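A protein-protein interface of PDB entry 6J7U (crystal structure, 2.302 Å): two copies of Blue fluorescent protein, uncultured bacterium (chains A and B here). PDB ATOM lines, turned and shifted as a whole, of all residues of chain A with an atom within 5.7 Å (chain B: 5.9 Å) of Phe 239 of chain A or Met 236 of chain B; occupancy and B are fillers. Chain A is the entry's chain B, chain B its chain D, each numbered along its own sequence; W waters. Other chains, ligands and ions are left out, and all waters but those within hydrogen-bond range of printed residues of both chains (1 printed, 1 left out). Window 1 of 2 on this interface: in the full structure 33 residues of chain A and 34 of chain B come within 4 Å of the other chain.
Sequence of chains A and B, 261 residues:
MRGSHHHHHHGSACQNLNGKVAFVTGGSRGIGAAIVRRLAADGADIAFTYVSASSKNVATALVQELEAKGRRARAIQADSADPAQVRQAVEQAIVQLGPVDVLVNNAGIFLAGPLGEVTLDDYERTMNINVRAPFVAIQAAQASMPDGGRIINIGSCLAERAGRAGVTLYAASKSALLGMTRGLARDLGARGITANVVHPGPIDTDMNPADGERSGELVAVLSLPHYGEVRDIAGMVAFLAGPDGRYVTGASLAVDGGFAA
The backbone carbonyl oxygen of Pro 243 of chain A is in hydrogen-bond range of the guanidinium group of Arg 231 of chain B. NE of Arg 246 of chain A is in salt-bridge range of OD1 of Asp 232 of chain B (2.5 Å). The guanidinium group (NE) of Arg 231 of chain B sits close to the guanidinium group (NH1) of Arg 246 of chain A, 3.4 Å away.
The backbone carbonyl oxygen of Phe 239 of chain A sits at hydrogen-bond distance from the backbone NH of Gly 245 of chain A (3.3 Å).
Met 236 of chain A touches Phe 239 of chain B. Gly 235 of chain B touches Phe 239 of chain A. CE2 of Phe 239 of chain A touches CE of Met 236 of chain B, 3.5 Å away. CD1 of Phe 239 of chain A touches CB of Phe 239 of chain B (3.7 Å). Asp 244 of chain A touches Gly 235 of chain B (CG to CA, 3.9 Å). Val 248 of chain A touches Ala 254 of chain B (CG1 to O, 3.4 Å).
Printed residues of chain B within 4 Å of Phe 239 of chain A: Gly 235, Met 236 and Phe 239. Of chain A, only Phe 239 (3.5 Å) comes within 4 Å of Met 236 of chain B. Printed residues of chain A within 4 Å of Phe 239 of chain B: Met 236 (3.6 Å) and Phe 239 (3.7 Å). Printed residues of chain A within 4 Å of Asp 232 of chain B: Arg 246. Printed residues of chain A within 4 Å of Arg 231 of chain B: Pro 243 (2.9 Å) and Arg 246 (3.2 Å). Ala 234 of chain A touches none of the printed residues of chain B. Val 255 of chain B touches none of the printed residues of chain A. The nearest residue of chain A that does not touch Met 236 of chain B is Val 248 of chain A (4.3 Å). The nearest printed residue of chain B that does not touch Met 236 of chain A is Leu 253 of chain B (4.3 Å).
Of the 15 printed residues of chain B, 6 touch a printed residue of chain A. Along chain B the printed residues that touch a printed residue of chain A span positions 231 to 254.
Met 236 of chain A touches Phe 239 of chain B, and with the chains exchanged Phe 239 of chain A touches Met 236 of chain B. Phe 239 of chain A touches Gly 235 of chain B, but with the chains exchanged Gly 235 of chain A does not touch Phe 239 of chain B (4.002 Å). Phe 239 of chain A touches its own counterpart, Phe 239 of chain B. 9 positions are printed for both chains. Of the 9 pairs that touch across the chains among the printed residues, 3 have their exchanged pair printed and touching as well.
Water W1 lies within hydrogen-bond range of O of Asp 244 of chain A (2.6 Å), OD1 of Asp 232 of chain B (2.9 Å) and N of Arg 246 of chain A (3.3 Å).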
ATOM      1  N   ALA A 234       1.406 -18.343  -4.485  1.00  0.00           N
ATOM      2  CA  ALA A 234       0.811 -17.543  -3.427  1.00  0.00           C
ATOM      3  C   ALA A 234      -0.065 -16.443  -4.017  1.00  0.00           C
ATOM      4  O   ALA A 234      -1.193 -16.233  -3.553  1.00  0.00           O
ATOM      5  CB  ALA A 234       1.902 -16.961  -2.537  1.00  0.00           C
ATOM      6  N   GLY A 235       0.369 -15.826  -5.120  1.00  0.00           N
ATOM      7  CA  GLY A 235      -0.450 -14.792  -5.721  1.00  0.00           C
ATOM      8  C   GLY A 235      -1.750 -15.339  -6.288  1.00  0.00           C
ATOM      9  O   GLY A 235      -2.816 -14.738  -6.113  1.00  0.00           O
ATOM     10  N   MET A 236      -1.710 -16.513  -6.913  1.00  0.00           N
ATOM     11  CA  MET A 236      -2.967 -17.037  -7.395  1.00  0.00           C
ATOM     12  C   MET A 236      -3.883 -17.337  -6.229  1.00  0.00           C
ATOM     13  O   MET A 236      -5.080 -17.041  -6.296  1.00  0.00           O
ATOM     14  CB  MET A 236      -2.751 -18.279  -8.267  1.00  0.00           C
ATOM     15  CG  MET A 236      -4.052 -19.032  -8.595  1.00  0.00           C
ATOM     16  SD  MET A 236      -5.137 -18.080  -9.703  1.00  0.00           S
ATOM     17  CE  MET A 236      -4.221 -18.135 -11.248  1.00  0.00           C
ATOM     18  N   VAL A 237      -3.326 -17.859  -5.117  1.00  0.00           N
ATOM     19  CA  VAL A 237      -4.164 -18.162  -3.960  1.00  0.00           C
ATOM     20  C   VAL A 237      -4.761 -16.889  -3.380  1.00  0.00           C
ATOM     21  O   VAL A 237      -5.957 -16.825  -3.066  1.00  0.00           O
ATOM     22  CB  VAL A 237      -3.382 -18.960  -2.905  1.00  0.00           C
ATOM     23  CG1 VAL A 237      -4.179 -18.976  -1.587  1.00  0.00           C
ATOM     24  CG2 VAL A 237      -3.181 -20.398  -3.370  1.00  0.00           C
ATOM     25  N   ALA A 238      -3.961 -15.835  -3.277  1.00  0.00           N
ATOM     26  CA  ALA A 238      -4.478 -14.580  -2.745  1.00  0.00           C
ATOM     27  C   ALA A 238      -5.613 -14.027  -3.607  1.00  0.00           C
ATOM     28  O   ALA A 238      -6.603 -13.504  -3.094  1.00  0.00           O
ATOM     29  CB  ALA A 238      -3.344 -13.566  -2.668  1.00  0.00           C
ATOM     30  N   PHE A 239      -5.498 -14.156  -4.918  1.00  0.00           N
ATOM     31  CA  PHE A 239      -6.565 -13.667  -5.777  1.00  0.00           C
ATOM     32  C   PHE A 239      -7.862 -14.425  -5.500  1.00  0.00           C
ATOM     33  O   PHE A 239      -8.938 -13.818  -5.424  1.00  0.00           O
ATOM     34  CB  PHE A 239      -6.130 -13.788  -7.242  1.00  0.00           C
ATOM     35  CG  PHE A 239      -7.262 -13.663  -8.237  1.00  0.00           C
ATOM     36  CD1 PHE A 239      -7.684 -12.411  -8.682  1.00  0.00           C
ATOM     37  CD2 PHE A 239      -7.881 -14.779  -8.744  1.00  0.00           C
ATOM     38  CE1 PHE A 239      -8.711 -12.276  -9.600  1.00  0.00           C
ATOM     39  CE2 PHE A 239      -8.911 -14.645  -9.638  1.00  0.00           C
ATOM     40  CZ  PHE A 239      -9.332 -13.364 -10.076  1.00  0.00           C
ATOM     41  N   LEU A 240      -7.782 -15.752  -5.322  1.00  0.00           N
ATOM     42  CA  LEU A 240      -9.008 -16.513  -5.065  1.00  0.00           C
ATOM     43  C   LEU A 240      -9.564 -16.227  -3.686  1.00  0.00           C
ATOM     44  O   LEU A 240     -10.787 -16.143  -3.519  1.00  0.00           O
ATOM     45  CB  LEU A 240      -8.766 -18.016  -5.217  1.00  0.00           C
ATOM     46  CG  LEU A 240      -8.330 -18.428  -6.623  1.00  0.00           C
ATOM     47  CD1 LEU A 240      -7.702 -19.815  -6.693  1.00  0.00           C
ATOM     48  CD2 LEU A 240      -9.456 -18.272  -7.624  1.00  0.00           C
ATOM     49  N   ALA A 241      -8.689 -15.989  -2.717  1.00  0.00           N
ATOM     50  CA  ALA A 241      -9.140 -15.743  -1.359  1.00  0.00           C
ATOM     51  C   ALA A 241      -9.861 -14.418  -1.216  1.00  0.00           C
ATOM     52  O   ALA A 241     -10.681 -14.277  -0.308  1.00  0.00           O
ATOM     53  CB  ALA A 241      -7.954 -15.752  -0.385  1.00  0.00           C
ATOM     54  N   GLY A 242      -9.531 -13.418  -2.047  1.00  0.00           N
ATOM     55  CA  GLY A 242     -10.000 -12.057  -1.865  1.00  0.00           C
ATOM     56  C   GLY A 242     -11.214 -11.634  -2.676  1.00  0.00           C
ATOM     57  O   GLY A 242     -11.868 -12.435  -3.334  1.00  0.00           O
ATOM     58  N   PRO A 243     -11.491 -10.328  -2.685  1.00  0.00           N
ATOM     59  CA  PRO A 243     -12.687  -9.819  -3.367  1.00  0.00           C
ATOM     60  C   PRO A 243     -12.751 -10.135  -4.835  1.00  0.00           C
ATOM     61  O   PRO A 243     -13.853 -10.204  -5.376  1.00  0.00           O
ATOM     62  CB  PRO A 243     -12.612  -8.309  -3.140  1.00  0.00           C
ATOM     63  CG  PRO A 243     -11.708  -8.153  -2.006  1.00  0.00           C
ATOM     64  CD  PRO A 243     -10.711  -9.246  -2.082  1.00  0.00           C
ATOM     65  N   ASP A 244     -11.624 -10.230  -5.521  1.00  0.00           N
ATOM     66  CA  ASP A 244     -11.705 -10.516  -6.947  1.00  0.00           C
ATOM     67  C   ASP A 244     -12.044 -11.967  -7.245  1.00  0.00           C
ATOM     68  O   ASP A 244     -12.416 -12.271  -8.381  1.00  0.00           O
ATOM     69  CB  ASP A 244     -10.396 -10.136  -7.655  1.00  0.00           C
ATOM     70  CG  ASP A 244     -10.222  -8.609  -7.797  1.00  0.00           C
ATOM     71  OD1 ASP A 244     -11.253  -7.889  -7.802  1.00  0.00           O
ATOM     72  OD2 ASP A 244      -9.056  -8.137  -7.885  1.00  0.00           O
ATOM     73  N   GLY A 245     -11.948 -12.863  -6.269  1.00  0.00           N
ATOM     74  CA  GLY A 245     -12.280 -14.232  -6.538  1.00  0.00           C
ATOM     75  C   GLY A 245     -13.729 -14.580  -6.338  1.00  0.00           C
ATOM     76  O   GLY A 245     -14.105 -15.741  -6.563  1.00  0.00           O
ATOM     77  N   ARG A 246     -14.557 -13.595  -5.957  1.00  0.00           N
ATOM     78  CA  ARG A 246     -15.884 -13.881  -5.396  1.00  0.00           C
ATOM     79  C   ARG A 246     -16.796 -14.611  -6.368  1.00  0.00           C
ATOM     80  O   ARG A 246     -17.745 -15.263  -5.932  1.00  0.00           O
ATOM     81  CB  ARG A 246     -16.576 -12.597  -4.959  1.00  0.00           C
ATOM     82  CG  ARG A 246     -16.873 -11.693  -6.152  1.00  0.00           C
ATOM     83  CD  ARG A 246     -17.666 -10.477  -5.740  1.00  0.00           C
ATOM     84  NE  ARG A 246     -18.093  -9.674  -6.875  1.00  0.00           N
ATOM     85  CZ  ARG A 246     -18.941  -8.647  -6.765  1.00  0.00           C
ATOM     86  NH1 ARG A 246     -19.290  -7.946  -7.841  1.00  0.00           N
ATOM     87  NH2 ARG A 246     -19.485  -8.349  -5.578  1.00  0.00           N
ATOM     88  N   VAL A 248     -15.479 -16.639  -8.951  1.00  0.00           N
ATOM     89  CA  VAL A 248     -14.754 -17.778  -9.507  1.00  0.00           C
ATOM     90  C   VAL A 248     -15.055 -19.015  -8.656  1.00  0.00           C
ATOM     91  O   VAL A 248     -14.786 -19.021  -7.439  1.00  0.00           O
ATOM     92  CB  VAL A 248     -13.245 -17.490  -9.547  1.00  0.00           C
ATOM     93  CG1 VAL A 248     -12.488 -18.624 -10.330  1.00  0.00           C
ATOM     94  CG2 VAL A 248     -13.000 -16.135 -10.126  1.00  0.00           C
ATOM     95  N   LEU A 253      -7.264 -23.758 -12.226  1.00  0.00           N
ATOM     96  CA  LEU A 253      -6.454 -22.618 -12.636  1.00  0.00           C
ATOM     97  C   LEU A 253      -4.988 -23.013 -12.751  1.00  0.00           C
ATOM     98  O   LEU A 253      -4.323 -23.253 -11.742  1.00  0.00           O
ATOM     99  CB  LEU A 253      -6.664 -21.493 -11.653  1.00  0.00           C
ATOM    100  CG  LEU A 253      -8.143 -21.119 -11.567  1.00  0.00           C
ATOM    101  CD1 LEU A 253      -8.819 -21.884 -10.412  1.00  0.00           C
ATOM    102  CD2 LEU A 253      -8.282 -19.637 -11.347  1.00  0.00           C
ATOM    103  N   VAL B 198     -10.097 -15.584 -20.767  1.00  0.00           N
ATOM    104  CA  VAL B 198     -11.008 -15.537 -19.628  1.00  0.00           C
ATOM    105  C   VAL B 198     -12.410 -15.859 -20.122  1.00  0.00           C
ATOM    106  O   VAL B 198     -12.916 -15.205 -21.052  1.00  0.00           O
ATOM    107  CB  VAL B 198     -10.994 -14.160 -18.934  1.00  0.00           C
ATOM    108  CG1 VAL B 198     -12.054 -14.106 -17.816  1.00  0.00           C
ATOM    109  CG2 VAL B 198      -9.585 -13.865 -18.390  1.00  0.00           C
ATOM    110  N   ARG B 231     -17.209  -5.927 -12.699  1.00  0.00           N
ATOM    111  CA  ARG B 231     -15.973  -5.939 -11.895  1.00  0.00           C
ATOM    112  C   ARG B 231     -15.385  -7.334 -11.717  1.00  0.00           C
ATOM    113  O   ARG B 231     -14.162  -7.474 -11.570  1.00  0.00           O
ATOM    114  CB  ARG B 231     -16.169  -5.351 -10.493  1.00  0.00           C
ATOM    115  CG  ARG B 231     -17.301  -5.907  -9.674  1.00  0.00           C
ATOM    116  CD  ARG B 231     -17.102  -5.649  -8.151  1.00  0.00           C
ATOM    117  NE  ARG B 231     -16.170  -6.603  -7.524  1.00  0.00           N
ATOM    118  CZ  ARG B 231     -15.775  -6.567  -6.247  1.00  0.00           C
ATOM    119  NH1 ARG B 231     -14.946  -7.503  -5.764  1.00  0.00           N
ATOM    120  NH2 ARG B 231     -16.175  -5.568  -5.457  1.00  0.00           N
ATOM    121  N   ASP B 232     -16.206  -8.379 -11.728  1.00  0.00           N
ATOM    122  CA  ASP B 232     -15.617  -9.705 -11.573  1.00  0.00           C
ATOM    123  C   ASP B 232     -14.715 -10.045 -12.760  1.00  0.00           C
ATOM    124  O   ASP B 232     -13.677 -10.709 -12.595  1.00  0.00           O
ATOM    125  CB  ASP B 232     -16.717 -10.754 -11.405  1.00  0.00           C
ATOM    126  CG  ASP B 232     -17.563 -10.510 -10.165  1.00  0.00           C
ATOM    127  OD1 ASP B 232     -17.003 -10.410  -9.053  1.00  0.00           O
ATOM    128  OD2 ASP B 232     -18.794 -10.370 -10.314  1.00  0.00           O
ATOM    129  N   ILE B 233     -15.092  -9.603 -13.971  1.00  0.00           N
ATOM    130  CA  ILE B 233     -14.230  -9.846 -15.125  1.00  0.00           C
ATOM    131  C   ILE B 233     -13.033  -8.900 -15.103  1.00  0.00           C
ATOM    132  O   ILE B 233     -11.897  -9.300 -15.391  1.00  0.00           O
ATOM    133  CB  ILE B 233     -15.021  -9.721 -16.460  1.00  0.00           C
ATOM    134  CG1 ILE B 233     -16.250 -10.642 -16.470  1.00  0.00           C
ATOM    135  CG2 ILE B 233     -14.139 -10.064 -17.640  1.00  0.00           C
ATOM    136  CD1 ILE B 233     -15.891 -12.157 -16.066  1.00  0.00           C
ATOM    137  N   ALA B 234     -13.253  -7.636 -14.767  1.00  0.00           N
ATOM    138  CA  ALA B 234     -12.127  -6.708 -14.763  1.00  0.00           C
ATOM    139  C   ALA B 234     -11.085  -7.165 -13.757  1.00  0.00           C
ATOM    140  O   ALA B 234      -9.882  -7.099 -14.024  1.00  0.00           O
ATOM    141  CB  ALA B 234     -12.603  -5.276 -14.469  1.00  0.00           C
ATOM    142  N   GLY B 235     -11.520  -7.716 -12.624  1.00  0.00           N
ATOM    143  CA  GLY B 235     -10.543  -8.161 -11.647  1.00  0.00           C
ATOM    144  C   GLY B 235      -9.674  -9.309 -12.146  1.00  0.00           C
ATOM    145  O   GLY B 235      -8.452  -9.286 -11.968  1.00  0.00           O
ATOM    146  N   MET B 236     -10.269 -10.303 -12.829  1.00  0.00           N
ATOM    147  CA  MET B 236      -9.437 -11.375 -13.363  1.00  0.00           C
ATOM    148  C   MET B 236      -8.463 -10.843 -14.426  1.00  0.00           C
ATOM    149  O   MET B 236      -7.281 -11.232 -14.447  1.00  0.00           O
ATOM    150  CB  MET B 236     -10.332 -12.484 -13.911  1.00  0.00           C
ATOM    151  CG  MET B 236      -9.639 -13.496 -14.753  1.00  0.00           C
ATOM    152  SD  MET B 236      -8.523 -14.551 -13.822  1.00  0.00           S
ATOM    153  CE  MET B 236      -9.744 -15.476 -12.910  1.00  0.00           C
ATOM    154  N   VAL B 237      -8.912  -9.920 -15.298  1.00  0.00           N
ATOM    155  CA  VAL B 237      -7.970  -9.378 -16.277  1.00  0.00           C
ATOM    156  C   VAL B 237      -6.864  -8.608 -15.562  1.00  0.00           C
ATOM    157  O   VAL B 237      -5.684  -8.806 -15.833  1.00  0.00           O
ATOM    158  CB  VAL B 237      -8.675  -8.475 -17.310  1.00  0.00           C
ATOM    159  CG1 VAL B 237      -7.644  -7.802 -18.269  1.00  0.00           C
ATOM    160  CG2 VAL B 237      -9.784  -9.220 -18.092  1.00  0.00           C
ATOM    161  N   ALA B 238      -7.218  -7.789 -14.579  1.00  0.00           N
ATOM    162  CA  ALA B 238      -6.183  -7.040 -13.879  1.00  0.00           C
ATOM    163  C   ALA B 238      -5.181  -7.984 -13.219  1.00  0.00           C
ATOM    164  O   ALA B 238      -3.964  -7.782 -13.331  1.00  0.00           O
ATOM    165  CB  ALA B 238      -6.824  -6.120 -12.827  1.00  0.00           C
ATOM    166  N   PHE B 239      -5.643  -9.086 -12.661  1.00  0.00           N
ATOM    167  CA  PHE B 239      -4.745 -10.069 -12.102  1.00  0.00           C
ATOM    168  C   PHE B 239      -3.799 -10.634 -13.160  1.00  0.00           C
ATOM    169  O   PHE B 239      -2.659 -10.751 -12.918  1.00  0.00           O
ATOM    170  CB  PHE B 239      -5.527 -11.192 -11.427  1.00  0.00           C
ATOM    171  CG  PHE B 239      -4.746 -12.414 -11.197  1.00  0.00           C
ATOM    172  CD1 PHE B 239      -3.909 -12.511 -10.137  1.00  0.00           C
ATOM    173  CD2 PHE B 239      -4.804 -13.435 -12.071  1.00  0.00           C
ATOM    174  CE1 PHE B 239      -3.147 -13.609  -9.938  1.00  0.00           C
ATOM    175  CE2 PHE B 239      -4.042 -14.550 -11.883  1.00  0.00           C
ATOM    176  CZ  PHE B 239      -3.219 -14.641 -10.811  1.00  0.00           C
ATOM    177  N   LEU B 240      -4.286 -10.950 -14.332  1.00  0.00           N
ATOM    178  CA  LEU B 240      -3.483 -11.473 -15.399  1.00  0.00           C
ATOM    179  C   LEU B 240      -2.476 -10.501 -15.944  1.00  0.00           C
ATOM    180  O   LEU B 240      -1.460 -10.878 -16.390  1.00  0.00           O
ATOM    181  CB  LEU B 240      -4.306 -12.071 -16.504  1.00  0.00           C
ATOM    182  CG  LEU B 240      -4.961 -13.368 -16.172  1.00  0.00           C
ATOM    183  CD1 LEU B 240      -6.177 -13.658 -17.002  1.00  0.00           C
ATOM    184  CD2 LEU B 240      -3.949 -14.448 -16.239  1.00  0.00           C
ATOM    185  N   ALA B 241      -2.865  -9.254 -15.993  1.00  0.00           N
ATOM    186  CA  ALA B 241      -2.038  -8.191 -16.432  1.00  0.00           C
ATOM    187  C   ALA B 241      -0.885  -7.837 -15.504  1.00  0.00           C
ATOM    188  O   ALA B 241       0.125  -7.372 -15.954  1.00  0.00           O
ATOM    189  CB  ALA B 241      -2.873  -6.977 -16.726  1.00  0.00           C
ATOM    190  N   LEU B 253      -9.258 -19.467 -17.934  1.00  0.00           N
ATOM    191  CA  LEU B 253      -9.629 -19.077 -16.579  1.00  0.00           C
ATOM    192  C   LEU B 253     -11.106 -18.712 -16.582  1.00  0.00           C
ATOM    193  O   LEU B 253     -11.501 -17.708 -17.192  1.00  0.00           O
ATOM    194  CB  LEU B 253      -8.775 -17.912 -16.071  1.00  0.00           C
ATOM    195  CG  LEU B 253      -7.277 -18.111 -15.976  1.00  0.00           C
ATOM    196  CD1 LEU B 253      -6.533 -17.600 -17.196  1.00  0.00           C
ATOM    197  CD2 LEU B 253      -6.736 -17.441 -14.709  1.00  0.00           C
ATOM    198  N   ALA B 254     -11.924 -19.552 -15.941  1.00  0.00           N
ATOM    199  CA  ALA B 254     -13.364 -19.343 -15.874  1.00  0.00           C
ATOM    200  C   ALA B 254     -13.745 -18.445 -14.709  1.00  0.00           C
ATOM    201  O   ALA B 254     -13.424 -18.746 -13.554  1.00  0.00           O
ATOM    202  CB  ALA B 254     -14.108 -20.666 -15.736  1.00  0.00           C
ATOM    203  N   VAL B 255     -14.515 -17.399 -15.010  1.00  0.00           N
ATOM    204  CA  VAL B 255     -15.127 -16.528 -14.020  1.00  0.00           C
ATOM    205  C   VAL B 255     -16.626 -16.655 -14.230  1.00  0.00           C
ATOM    206  O   VAL B 255     -17.265 -15.710 -14.713  1.00  0.00           O
ATOM    207  CB  VAL B 255     -14.684 -15.061 -14.185  1.00  0.00           C
ATOM    208  CG1 VAL B 255     -15.216 -14.227 -13.050  1.00  0.00           C
ATOM    209  CG2 VAL B 255     -13.180 -14.948 -14.292  1.00  0.00           C
HETATM  210  O   HOH W   1     -14.957 -12.494  -9.047  1.00  0.00           O
